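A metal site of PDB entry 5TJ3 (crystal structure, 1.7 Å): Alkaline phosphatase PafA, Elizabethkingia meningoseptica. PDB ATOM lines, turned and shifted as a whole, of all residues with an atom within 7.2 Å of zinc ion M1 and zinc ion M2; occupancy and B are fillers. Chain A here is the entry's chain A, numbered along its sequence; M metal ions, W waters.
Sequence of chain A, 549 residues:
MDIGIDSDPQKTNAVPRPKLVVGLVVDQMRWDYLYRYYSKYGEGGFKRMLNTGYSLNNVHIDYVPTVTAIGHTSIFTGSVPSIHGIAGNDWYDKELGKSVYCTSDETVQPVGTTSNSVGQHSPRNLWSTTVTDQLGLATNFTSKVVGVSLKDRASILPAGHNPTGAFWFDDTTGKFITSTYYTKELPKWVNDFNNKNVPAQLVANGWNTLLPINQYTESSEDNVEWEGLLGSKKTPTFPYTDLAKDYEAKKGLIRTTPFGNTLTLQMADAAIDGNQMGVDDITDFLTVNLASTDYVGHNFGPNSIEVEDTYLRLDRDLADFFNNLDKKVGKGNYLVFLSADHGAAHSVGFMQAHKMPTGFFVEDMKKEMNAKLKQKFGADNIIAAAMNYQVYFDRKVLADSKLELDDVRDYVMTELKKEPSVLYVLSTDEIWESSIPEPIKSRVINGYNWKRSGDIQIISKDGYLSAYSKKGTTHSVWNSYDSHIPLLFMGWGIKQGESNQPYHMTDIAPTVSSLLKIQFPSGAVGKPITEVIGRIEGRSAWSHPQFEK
Of the 27 residues printed, 5 come within 4 Å of zinc ion M1.
Residues that only touch zinc ion M2: Gln 28 (3.98 Å). Of the 27 residues printed, 6 come within 4 Å of zinc ion M2. The nearest printed residue that does not touch zinc ion M2 is Lys 151 (4.5 Å).
Zinc ion M1 is bound by OD1 of Asp 27 (2.0 Å), OG1 of TPO 68 (2.0 Å), OD2 of Asp 341 (2.0 Å) and NE2 of His 342 (2.1 Å). Slightly farther from zinc ion M1 lies O3P of TPO 68 (2.8 Å).
A ring nitrogen (NE2) of His 342 lies close to a ring nitrogen (ND1) of His 475. A ring nitrogen (ND1) of His 475 sits at hydrogen-bond distance from the backbone carbonyl oxygen (O) of Thr 66. A ring nitrogen (ND1) of His 298 lies within hydrogen-bond range of the backbone carbonyl oxygen of Thr 473. The backbone carbonyl oxygen (O) of Asp 294 sits at hydrogen-bond distance from the side-chain amide nitrogen (NE2) of Gln 28 (3.2 Å). O of His 342 lies within hydrogen-bond range of N of Met 29, at 3.3 Å. The side-chain carboxylate (OD2) of Asp 27 is in hydrogen-bond range of the side-chain amide nitrogen (ND2) of Asn 289 (3.3 Å). N of Gln 28 is in hydrogen-bond range of OD1 of Asp 341 (3.2 Å). O2P of TPO 68 lies within salt-bridge range of NE of Arg 153 (3.0 Å).
Zinc ion M2 is bound by O3P of TPO 68 (1.9 Å), NE2 of His 298 (2.0 Å), NE2 of His 475 (2.2 Å), OD1 of Asp 294 (2.2 Å) and water W1 (2.4 Å). Zinc ion M2 has five donor atoms within binding distance. Slightly farther from zinc ion M2 lies OD2 of Asp 294 (2.7 Å).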
ATOM      1  N   VAL A  25      -7.219 -19.189 -11.578  1.00  0.00           N
ATOM      2  CA  VAL A  25      -7.460 -20.607 -11.772  1.00  0.00           C
ATOM      3  C   VAL A  25      -6.477 -21.371 -10.890  1.00  0.00           C
ATOM      4  O   VAL A  25      -5.255 -21.261 -11.050  1.00  0.00           O
ATOM      5  CB  VAL A  25      -7.373 -21.020 -13.251  1.00  0.00           C
ATOM      6  CG1 VAL A  25      -6.816 -19.909 -14.117  1.00  0.00           C
ATOM      7  CG2 VAL A  25      -6.668 -22.359 -13.449  1.00  0.00           C
ATOM      8  N   VAL A  26      -7.026 -22.095  -9.911  1.00  0.00           N
ATOM      9  CA  VAL A  26      -6.239 -22.852  -8.949  1.00  0.00           C
ATOM     10  C   VAL A  26      -5.939 -24.204  -9.583  1.00  0.00           C
ATOM     11  O   VAL A  26      -6.844 -25.010  -9.827  1.00  0.00           O
ATOM     12  CB  VAL A  26      -6.985 -23.030  -7.624  1.00  0.00           C
ATOM     13  CG1 VAL A  26      -6.126 -23.801  -6.633  1.00  0.00           C
ATOM     14  CG2 VAL A  26      -7.370 -21.667  -7.068  1.00  0.00           C
ATOM     15  N   ASP A  27      -4.667 -24.448  -9.865  1.00  0.00           N
ATOM     16  CA  ASP A  27      -4.276 -25.603 -10.652  1.00  0.00           C
ATOM     17  C   ASP A  27      -4.558 -26.890  -9.886  1.00  0.00           C
ATOM     18  O   ASP A  27      -4.135 -27.054  -8.739  1.00  0.00           O
ATOM     19  CB  ASP A  27      -2.798 -25.490 -11.014  1.00  0.00           C
ATOM     20  CG  ASP A  27      -2.457 -26.232 -12.271  1.00  0.00           C
ATOM     21  OD1 ASP A  27      -2.944 -27.369 -12.412  1.00  0.00           O
ATOM     22  OD2 ASP A  27      -1.718 -25.679 -13.109  1.00  0.00           O
ATOM     23  N   GLN A  28      -5.307 -27.797 -10.522  1.00  0.00           N
ATOM     24  CA  GLN A  28      -5.662 -29.115  -9.998  1.00  0.00           C
ATOM     25  C   GLN A  28      -6.655 -29.049  -8.840  1.00  0.00           C
ATOM     26  O   GLN A  28      -6.744 -29.990  -8.048  1.00  0.00           O
ATOM     27  CB  GLN A  28      -4.415 -29.911  -9.564  1.00  0.00           C
ATOM     28  CG  GLN A  28      -4.585 -31.418  -9.662  1.00  0.00           C
ATOM     29  CD  GLN A  28      -3.436 -32.177  -9.010  1.00  0.00           C
ATOM     30  OE1 GLN A  28      -3.597 -32.718  -7.912  1.00  0.00           O
ATOM     31  NE2 GLN A  28      -2.290 -32.217  -9.677  1.00  0.00           N
ATOM     32  N   MET A  29      -7.414 -27.963  -8.712  1.00  0.00           N
ATOM     33  CA  MET A  29      -8.353 -27.852  -7.592  1.00  0.00           C
ATOM     34  C   MET A  29      -9.628 -28.608  -7.920  1.00  0.00           C
ATOM     35  O   MET A  29     -10.453 -28.150  -8.705  1.00  0.00           O
ATOM     36  CB  MET A  29      -8.650 -26.390  -7.282  1.00  0.00           C
ATOM     37  CG  MET A  29      -9.582 -26.255  -6.106  1.00  0.00           C
ATOM     38  SD  MET A  29      -9.824 -24.547  -5.599  1.00  0.00           S
ATOM     39  CE  MET A  29     -10.889 -24.798  -4.181  1.00  0.00           C
ATOM     40  N   THR A  66      -8.052 -33.689 -19.722  1.00  0.00           N
ATOM     41  CA  THR A  66      -8.170 -32.629 -18.722  1.00  0.00           C
ATOM     42  C   THR A  66      -6.785 -32.290 -18.153  1.00  0.00           C
ATOM     43  O   THR A  66      -6.442 -32.605 -17.023  1.00  0.00           O
ATOM     44  CB  THR A  66      -9.155 -33.019 -17.634  1.00  0.00           C
ATOM     45  OG1 THR A  66      -8.834 -34.340 -17.149  1.00  0.00           O
ATOM     46  CG2 THR A  66     -10.574 -33.021 -18.175  1.00  0.00           C
ATOM     47  N   VAL A  67      -5.989 -31.624 -19.000  1.00  0.00           N
ATOM     48  CA  VAL A  67      -4.663 -31.178 -18.611  1.00  0.00           C
ATOM     49  C   VAL A  67      -4.587 -29.648 -18.578  1.00  0.00           C
ATOM     50  O   VAL A  67      -5.554 -28.973 -18.920  1.00  0.00           O
ATOM     51  CB  VAL A  67      -3.591 -31.758 -19.546  1.00  0.00           C
ATOM     52  CG1 VAL A  67      -3.670 -33.274 -19.549  1.00  0.00           C
ATOM     53  CG2 VAL A  67      -3.748 -31.203 -20.945  1.00  0.00           C
ATOM     54  N   TPO A  68      -3.433 -29.121 -18.177  1.00  0.00           N
ATOM     55  CA  TPO A  68      -3.262 -27.695 -17.885  1.00  0.00           C
ATOM     56  CB  TPO A  68      -1.927 -27.452 -17.214  1.00  0.00           C
ATOM     57  CG2 TPO A  68      -1.593 -25.962 -17.163  1.00  0.00           C
ATOM     58  OG1 TPO A  68      -2.007 -27.938 -15.892  1.00  0.00           O
ATOM     59  P   TPO A  68      -0.957 -29.157 -15.791  1.00  0.00           P
ATOM     60  O1P TPO A  68      -1.233 -30.189 -16.824  1.00  0.00           O
ATOM     61  O2P TPO A  68       0.524 -28.570 -16.003  1.00  0.00           O
ATOM     62  O3P TPO A  68      -1.110 -29.783 -14.326  1.00  0.00           O
ATOM     63  C   TPO A  68      -3.418 -26.763 -19.077  1.00  0.00           C
ATOM     64  O   TPO A  68      -4.222 -25.824 -19.036  1.00  0.00           O
ATOM     65  N   ALA A  69      -2.624 -26.998 -20.113  1.00  0.00           N
ATOM     66  CA  ALA A  69      -2.592 -26.106 -21.271  1.00  0.00           C
ATOM     67  C   ALA A  69      -3.989 -25.931 -21.840  1.00  0.00           C
ATOM     68  O   ALA A  69      -4.393 -24.813 -22.162  1.00  0.00           O
ATOM     69  CB  ALA A  69      -1.642 -26.619 -22.328  1.00  0.00           C
ATOM     70  N   GLY A  71      -6.892 -26.574 -20.239  1.00  0.00           N
ATOM     71  CA  GLY A  71      -7.770 -25.980 -19.241  1.00  0.00           C
ATOM     72  C   GLY A  71      -7.695 -24.465 -19.225  1.00  0.00           C
ATOM     73  O   GLY A  71      -8.719 -23.785 -19.278  1.00  0.00           O
ATOM     74  N   HIS A  72      -6.480 -23.928 -19.168  1.00  0.00           N
ATOM     75  CA  HIS A  72      -6.331 -22.472 -19.186  1.00  0.00           C
ATOM     76  C   HIS A  72      -6.781 -21.895 -20.519  1.00  0.00           C
ATOM     77  O   HIS A  72      -7.409 -20.829 -20.560  1.00  0.00           O
ATOM     78  CB  HIS A  72      -4.892 -22.096 -18.872  1.00  0.00           C
ATOM     79  CG  HIS A  72      -4.514 -22.295 -17.437  1.00  0.00           C
ATOM     80  ND1 HIS A  72      -4.190 -23.526 -16.912  1.00  0.00           N
ATOM     81  CD2 HIS A  72      -4.475 -21.424 -16.404  1.00  0.00           C
ATOM     82  CE1 HIS A  72      -3.935 -23.401 -15.628  1.00  0.00           C
ATOM     83  NE2 HIS A  72      -4.095 -22.133 -15.292  1.00  0.00           N
ATOM     84  N   ASN A  89      -0.748 -30.259 -23.121  1.00  0.00           N
ATOM     85  CA  ASN A  89       0.532 -29.664 -22.762  1.00  0.00           C
ATOM     86  C   ASN A  89       1.574 -29.943 -23.842  1.00  0.00           C
ATOM     87  O   ASN A  89       2.416 -29.107 -24.145  1.00  0.00           O
ATOM     88  CB  ASN A  89       1.020 -30.193 -21.420  1.00  0.00           C
ATOM     89  CG  ASN A  89       0.108 -29.801 -20.273  1.00  0.00           C
ATOM     90  OD1 ASN A  89      -0.576 -28.788 -20.329  1.00  0.00           O
ATOM     91  ND2 ASN A  89       0.095 -30.607 -19.212  1.00  0.00           N
ATOM     92  N   LYS A 151       4.145 -21.399 -14.137  1.00  0.00           N
ATOM     93  CA  LYS A 151       4.253 -22.161 -15.373  1.00  0.00           C
ATOM     94  C   LYS A 151       4.092 -21.237 -16.575  1.00  0.00           C
ATOM     95  O   LYS A 151       3.180 -20.405 -16.608  1.00  0.00           O
ATOM     96  CB  LYS A 151       3.195 -23.263 -15.455  1.00  0.00           C
ATOM     97  CG  LYS A 151       3.118 -24.207 -14.279  1.00  0.00           C
ATOM     98  CD  LYS A 151       1.946 -25.159 -14.480  1.00  0.00           C
ATOM     99  CE  LYS A 151       1.877 -26.211 -13.393  1.00  0.00           C
ATOM    100  NZ  LYS A 151       0.806 -27.215 -13.649  1.00  0.00           N
ATOM    101  N   ARG A 153       3.017 -22.043 -19.599  1.00  0.00           N
ATOM    102  CA  ARG A 153       1.753 -22.301 -20.301  1.00  0.00           C
ATOM    103  C   ARG A 153       0.581 -21.649 -19.585  1.00  0.00           C
ATOM    104  O   ARG A 153      -0.356 -21.158 -20.232  1.00  0.00           O
ATOM    105  CB  ARG A 153       1.533 -23.801 -20.451  1.00  0.00           C
ATOM    106  CG  ARG A 153       1.627 -24.611 -19.156  1.00  0.00           C
ATOM    107  CD  ARG A 153       1.530 -26.104 -19.446  1.00  0.00           C
ATOM    108  NE  ARG A 153       1.622 -26.937 -18.250  1.00  0.00           N
ATOM    109  CZ  ARG A 153       2.768 -27.395 -17.757  1.00  0.00           C
ATOM    110  NH1 ARG A 153       3.916 -27.101 -18.340  1.00  0.00           N
ATOM    111  NH2 ARG A 153       2.761 -28.155 -16.660  1.00  0.00           N
ATOM    112  N   ALA A 154       0.601 -21.632 -18.258  1.00  0.00           N
ATOM    113  CA  ALA A 154      -0.520 -21.111 -17.479  1.00  0.00           C
ATOM    114  C   ALA A 154      -0.506 -19.585 -17.362  1.00  0.00           C
ATOM    115  O   ALA A 154      -1.483 -19.015 -16.852  1.00  0.00           O
ATOM    116  CB  ALA A 154      -0.527 -21.737 -16.087  1.00  0.00           C
ATOM    117  N   ASN A 289      -2.540 -17.911 -12.414  1.00  0.00           N
ATOM    118  CA  ASN A 289      -2.678 -19.333 -12.137  1.00  0.00           C
ATOM    119  C   ASN A 289      -1.904 -19.657 -10.878  1.00  0.00           C
ATOM    120  O   ASN A 289      -0.740 -19.261 -10.739  1.00  0.00           O
ATOM    121  CB  ASN A 289      -2.164 -20.156 -13.316  1.00  0.00           C
ATOM    122  CG  ASN A 289      -1.644 -21.520 -12.891  1.00  0.00           C
ATOM    123  OD1 ASN A 289      -0.466 -21.672 -12.568  1.00  0.00           O
ATOM    124  ND2 ASN A 289      -2.519 -22.508 -12.903  1.00  0.00           N
ATOM    125  N   ALA A 291      -0.165 -22.437  -9.303  1.00  0.00           N
ATOM    126  CA  ALA A 291       0.326 -23.708  -9.801  1.00  0.00           C
ATOM    127  C   ALA A 291       0.730 -24.691  -8.707  1.00  0.00           C
ATOM    128  O   ALA A 291       0.771 -25.906  -8.971  1.00  0.00           O
ATOM    129  CB  ALA A 291       1.510 -23.493 -10.738  1.00  0.00           C
ATOM    130  N   ASP A 294      -1.064 -27.860  -7.875  1.00  0.00           N
ATOM    131  CA  ASP A 294      -0.875 -28.951  -8.833  1.00  0.00           C
ATOM    132  C   ASP A 294       0.410 -29.714  -8.570  1.00  0.00           C
ATOM    133  O   ASP A 294       0.428 -30.942  -8.597  1.00  0.00           O
ATOM    134  CB  ASP A 294      -0.871 -28.392 -10.255  1.00  0.00           C
ATOM    135  CG  ASP A 294      -0.692 -29.456 -11.303  1.00  0.00           C
ATOM    136  OD1 ASP A 294      -1.654 -30.220 -11.546  1.00  0.00           O
ATOM    137  OD2 ASP A 294       0.414 -29.530 -11.889  1.00  0.00           O
ATOM    138  N   TYR A 295       1.504 -28.992  -8.326  1.00  0.00           N
ATOM    139  CA  TYR A 295       2.775 -29.648  -8.020  1.00  0.00           C
ATOM    140  C   TYR A 295       2.659 -30.448  -6.731  1.00  0.00           C
ATOM    141  O   TYR A 295       3.070 -31.617  -6.672  1.00  0.00           O
ATOM    142  CB  TYR A 295       3.894 -28.616  -7.926  1.00  0.00           C
ATOM    143  CG  TYR A 295       4.319 -28.085  -9.268  1.00  0.00           C
ATOM    144  CD1 TYR A 295       5.124 -28.834 -10.110  1.00  0.00           C
ATOM    145  CD2 TYR A 295       3.922 -26.825  -9.701  1.00  0.00           C
ATOM    146  CE1 TYR A 295       5.518 -28.356 -11.348  1.00  0.00           C
ATOM    147  CE2 TYR A 295       4.308 -26.327 -10.932  1.00  0.00           C
ATOM    148  CZ  TYR A 295       5.112 -27.106 -11.748  1.00  0.00           C
ATOM    149  OH  TYR A 295       5.506 -26.636 -12.979  1.00  0.00           O
ATOM    150  N   HIS A 298       0.352 -33.444  -7.365  1.00  0.00           N
ATOM    151  CA  HIS A 298       1.006 -34.467  -8.168  1.00  0.00           C
ATOM    152  C   HIS A 298       1.918 -35.349  -7.327  1.00  0.00           C
ATOM    153  O   HIS A 298       2.049 -36.551  -7.577  1.00  0.00           O
ATOM    154  CB  HIS A 298       1.805 -33.823  -9.292  1.00  0.00           C
ATOM    155  CG  HIS A 298       1.032 -33.631 -10.563  1.00  0.00           C
ATOM    156  ND1 HIS A 298       0.607 -34.692 -11.333  1.00  0.00           N
ATOM    157  CD2 HIS A 298       0.623 -32.508 -11.191  1.00  0.00           C
ATOM    158  CE1 HIS A 298      -0.042 -34.219 -12.382  1.00  0.00           C
ATOM    159  NE2 HIS A 298      -0.044 -32.905 -12.320  1.00  0.00           N
ATOM    160  N   ALA A 340     -10.754 -23.847 -11.856  1.00  0.00           N
ATOM    161  CA  ALA A 340      -9.608 -24.727 -11.946  1.00  0.00           C
ATOM    162  C   ALA A 340      -9.509 -25.241 -13.371  1.00  0.00           C
ATOM    163  O   ALA A 340     -10.499 -25.276 -14.106  1.00  0.00           O
ATOM    164  CB  ALA A 340      -9.722 -25.904 -10.968  1.00  0.00           C
ATOM    165  N   ASP A 341      -8.301 -25.616 -13.766  1.00  0.00           N
ATOM    166  CA  ASP A 341      -8.118 -26.184 -15.102  1.00  0.00           C
ATOM    167  C   ASP A 341      -8.456 -27.661 -15.154  1.00  0.00           C
ATOM    168  O   ASP A 341      -8.590 -28.206 -16.260  1.00  0.00           O
ATOM    169  CB  ASP A 341      -6.683 -25.944 -15.577  1.00  0.00           C
ATOM    170  CG  ASP A 341      -5.640 -26.417 -14.582  1.00  0.00           C
ATOM    171  OD1 ASP A 341      -5.975 -26.655 -13.407  1.00  0.00           O
ATOM    172  OD2 ASP A 341      -4.465 -26.529 -14.985  1.00  0.00           O
ATOM    173  N   HIS A 342      -8.619 -28.305 -13.992  1.00  0.00           N
ATOM    174  CA  HIS A 342      -8.988 -29.709 -13.860  1.00  0.00           C
ATOM    175  C   HIS A 342      -8.973 -30.099 -12.387  1.00  0.00           C
ATOM    176  O   HIS A 342      -8.506 -29.335 -11.542  1.00  0.00           O
ATOM    177  CB  HIS A 342      -8.011 -30.605 -14.624  1.00  0.00           C
ATOM    178  CG  HIS A 342      -6.579 -30.327 -14.299  1.00  0.00           C
ATOM    179  ND1 HIS A 342      -6.005 -30.719 -13.103  1.00  0.00           N
ATOM    180  CD2 HIS A 342      -5.614 -29.653 -14.972  1.00  0.00           C
ATOM    181  CE1 HIS A 342      -4.749 -30.317 -13.075  1.00  0.00           C
ATOM    182  NE2 HIS A 342      -4.491 -29.666 -14.199  1.00  0.00           N
ATOM    183  N   GLY A 343      -9.497 -31.276 -12.068  1.00  0.00           N
ATOM    184  CA  GLY A 343      -9.383 -31.858 -10.745  1.00  0.00           C
ATOM    185  C   GLY A 343      -8.209 -32.811 -10.662  1.00  0.00           C
ATOM    186  O   GLY A 343      -7.158 -32.591 -11.283  1.00  0.00           O
ATOM    187  N   THR A 473      -0.409 -38.402  -7.727  1.00  0.00           N
ATOM    188  CA  THR A 473      -1.593 -38.577  -8.574  1.00  0.00           C
ATOM    189  C   THR A 473      -1.388 -37.803  -9.874  1.00  0.00           C
ATOM    190  O   THR A 473      -0.367 -37.155 -10.085  1.00  0.00           O
ATOM    191  CB  THR A 473      -2.869 -38.141  -7.844  1.00  0.00           C
ATOM    192  OG1 THR A 473      -4.006 -38.627  -8.556  1.00  0.00           O
ATOM    193  CG2 THR A 473      -2.932 -36.616  -7.759  1.00  0.00           C
ATOM    194  N   THR A 474      -2.391 -37.894 -10.746  1.00  0.00           N
ATOM    195  CA  THR A 474      -2.367 -37.196 -12.029  1.00  0.00           C
ATOM    196  C   THR A 474      -3.805 -36.981 -12.481  1.00  0.00           C
ATOM    197  O   THR A 474      -4.759 -37.282 -11.754  1.00  0.00           O
ATOM    198  CB  THR A 474      -1.535 -37.967 -13.058  1.00  0.00           C
ATOM    199  OG1 THR A 474      -1.350 -37.168 -14.228  1.00  0.00           O
ATOM    200  CG2 THR A 474      -2.232 -39.264 -13.438  1.00  0.00           C
ATOM    201  N   HIS A 475      -3.961 -36.485 -13.706  1.00  0.00           N
ATOM    202  CA  HIS A 475      -5.249 -36.004 -14.190  1.00  0.00           C
ATOM    203  C   HIS A 475      -5.212 -35.945 -15.715  1.00  0.00           C
ATOM    204  O   HIS A 475      -4.224 -35.471 -16.280  1.00  0.00           O
ATOM    205  CB  HIS A 475      -5.517 -34.606 -13.623  1.00  0.00           C
ATOM    206  CG  HIS A 475      -4.439 -33.631 -13.964  1.00  0.00           C
ATOM    207  ND1 HIS A 475      -4.358 -33.004 -15.191  1.00  0.00           N
ATOM    208  CD2 HIS A 475      -3.354 -33.220 -13.260  1.00  0.00           C
ATOM    209  CE1 HIS A 475      -3.298 -32.219 -15.220  1.00  0.00           C
ATOM    210  NE2 HIS A 475      -2.672 -32.337 -14.063  1.00  0.00           N
HETATM  211 ZN    ZN M   1      -3.222 -27.968 -14.263  1.00  0.00          ZN
HETATM  212 ZN    ZN M   2      -0.912 -31.345 -13.307  1.00  0.00          ZN
HETATM  213  O   HOH W   1       0.646 -31.744 -15.136  1.00  0.00           O
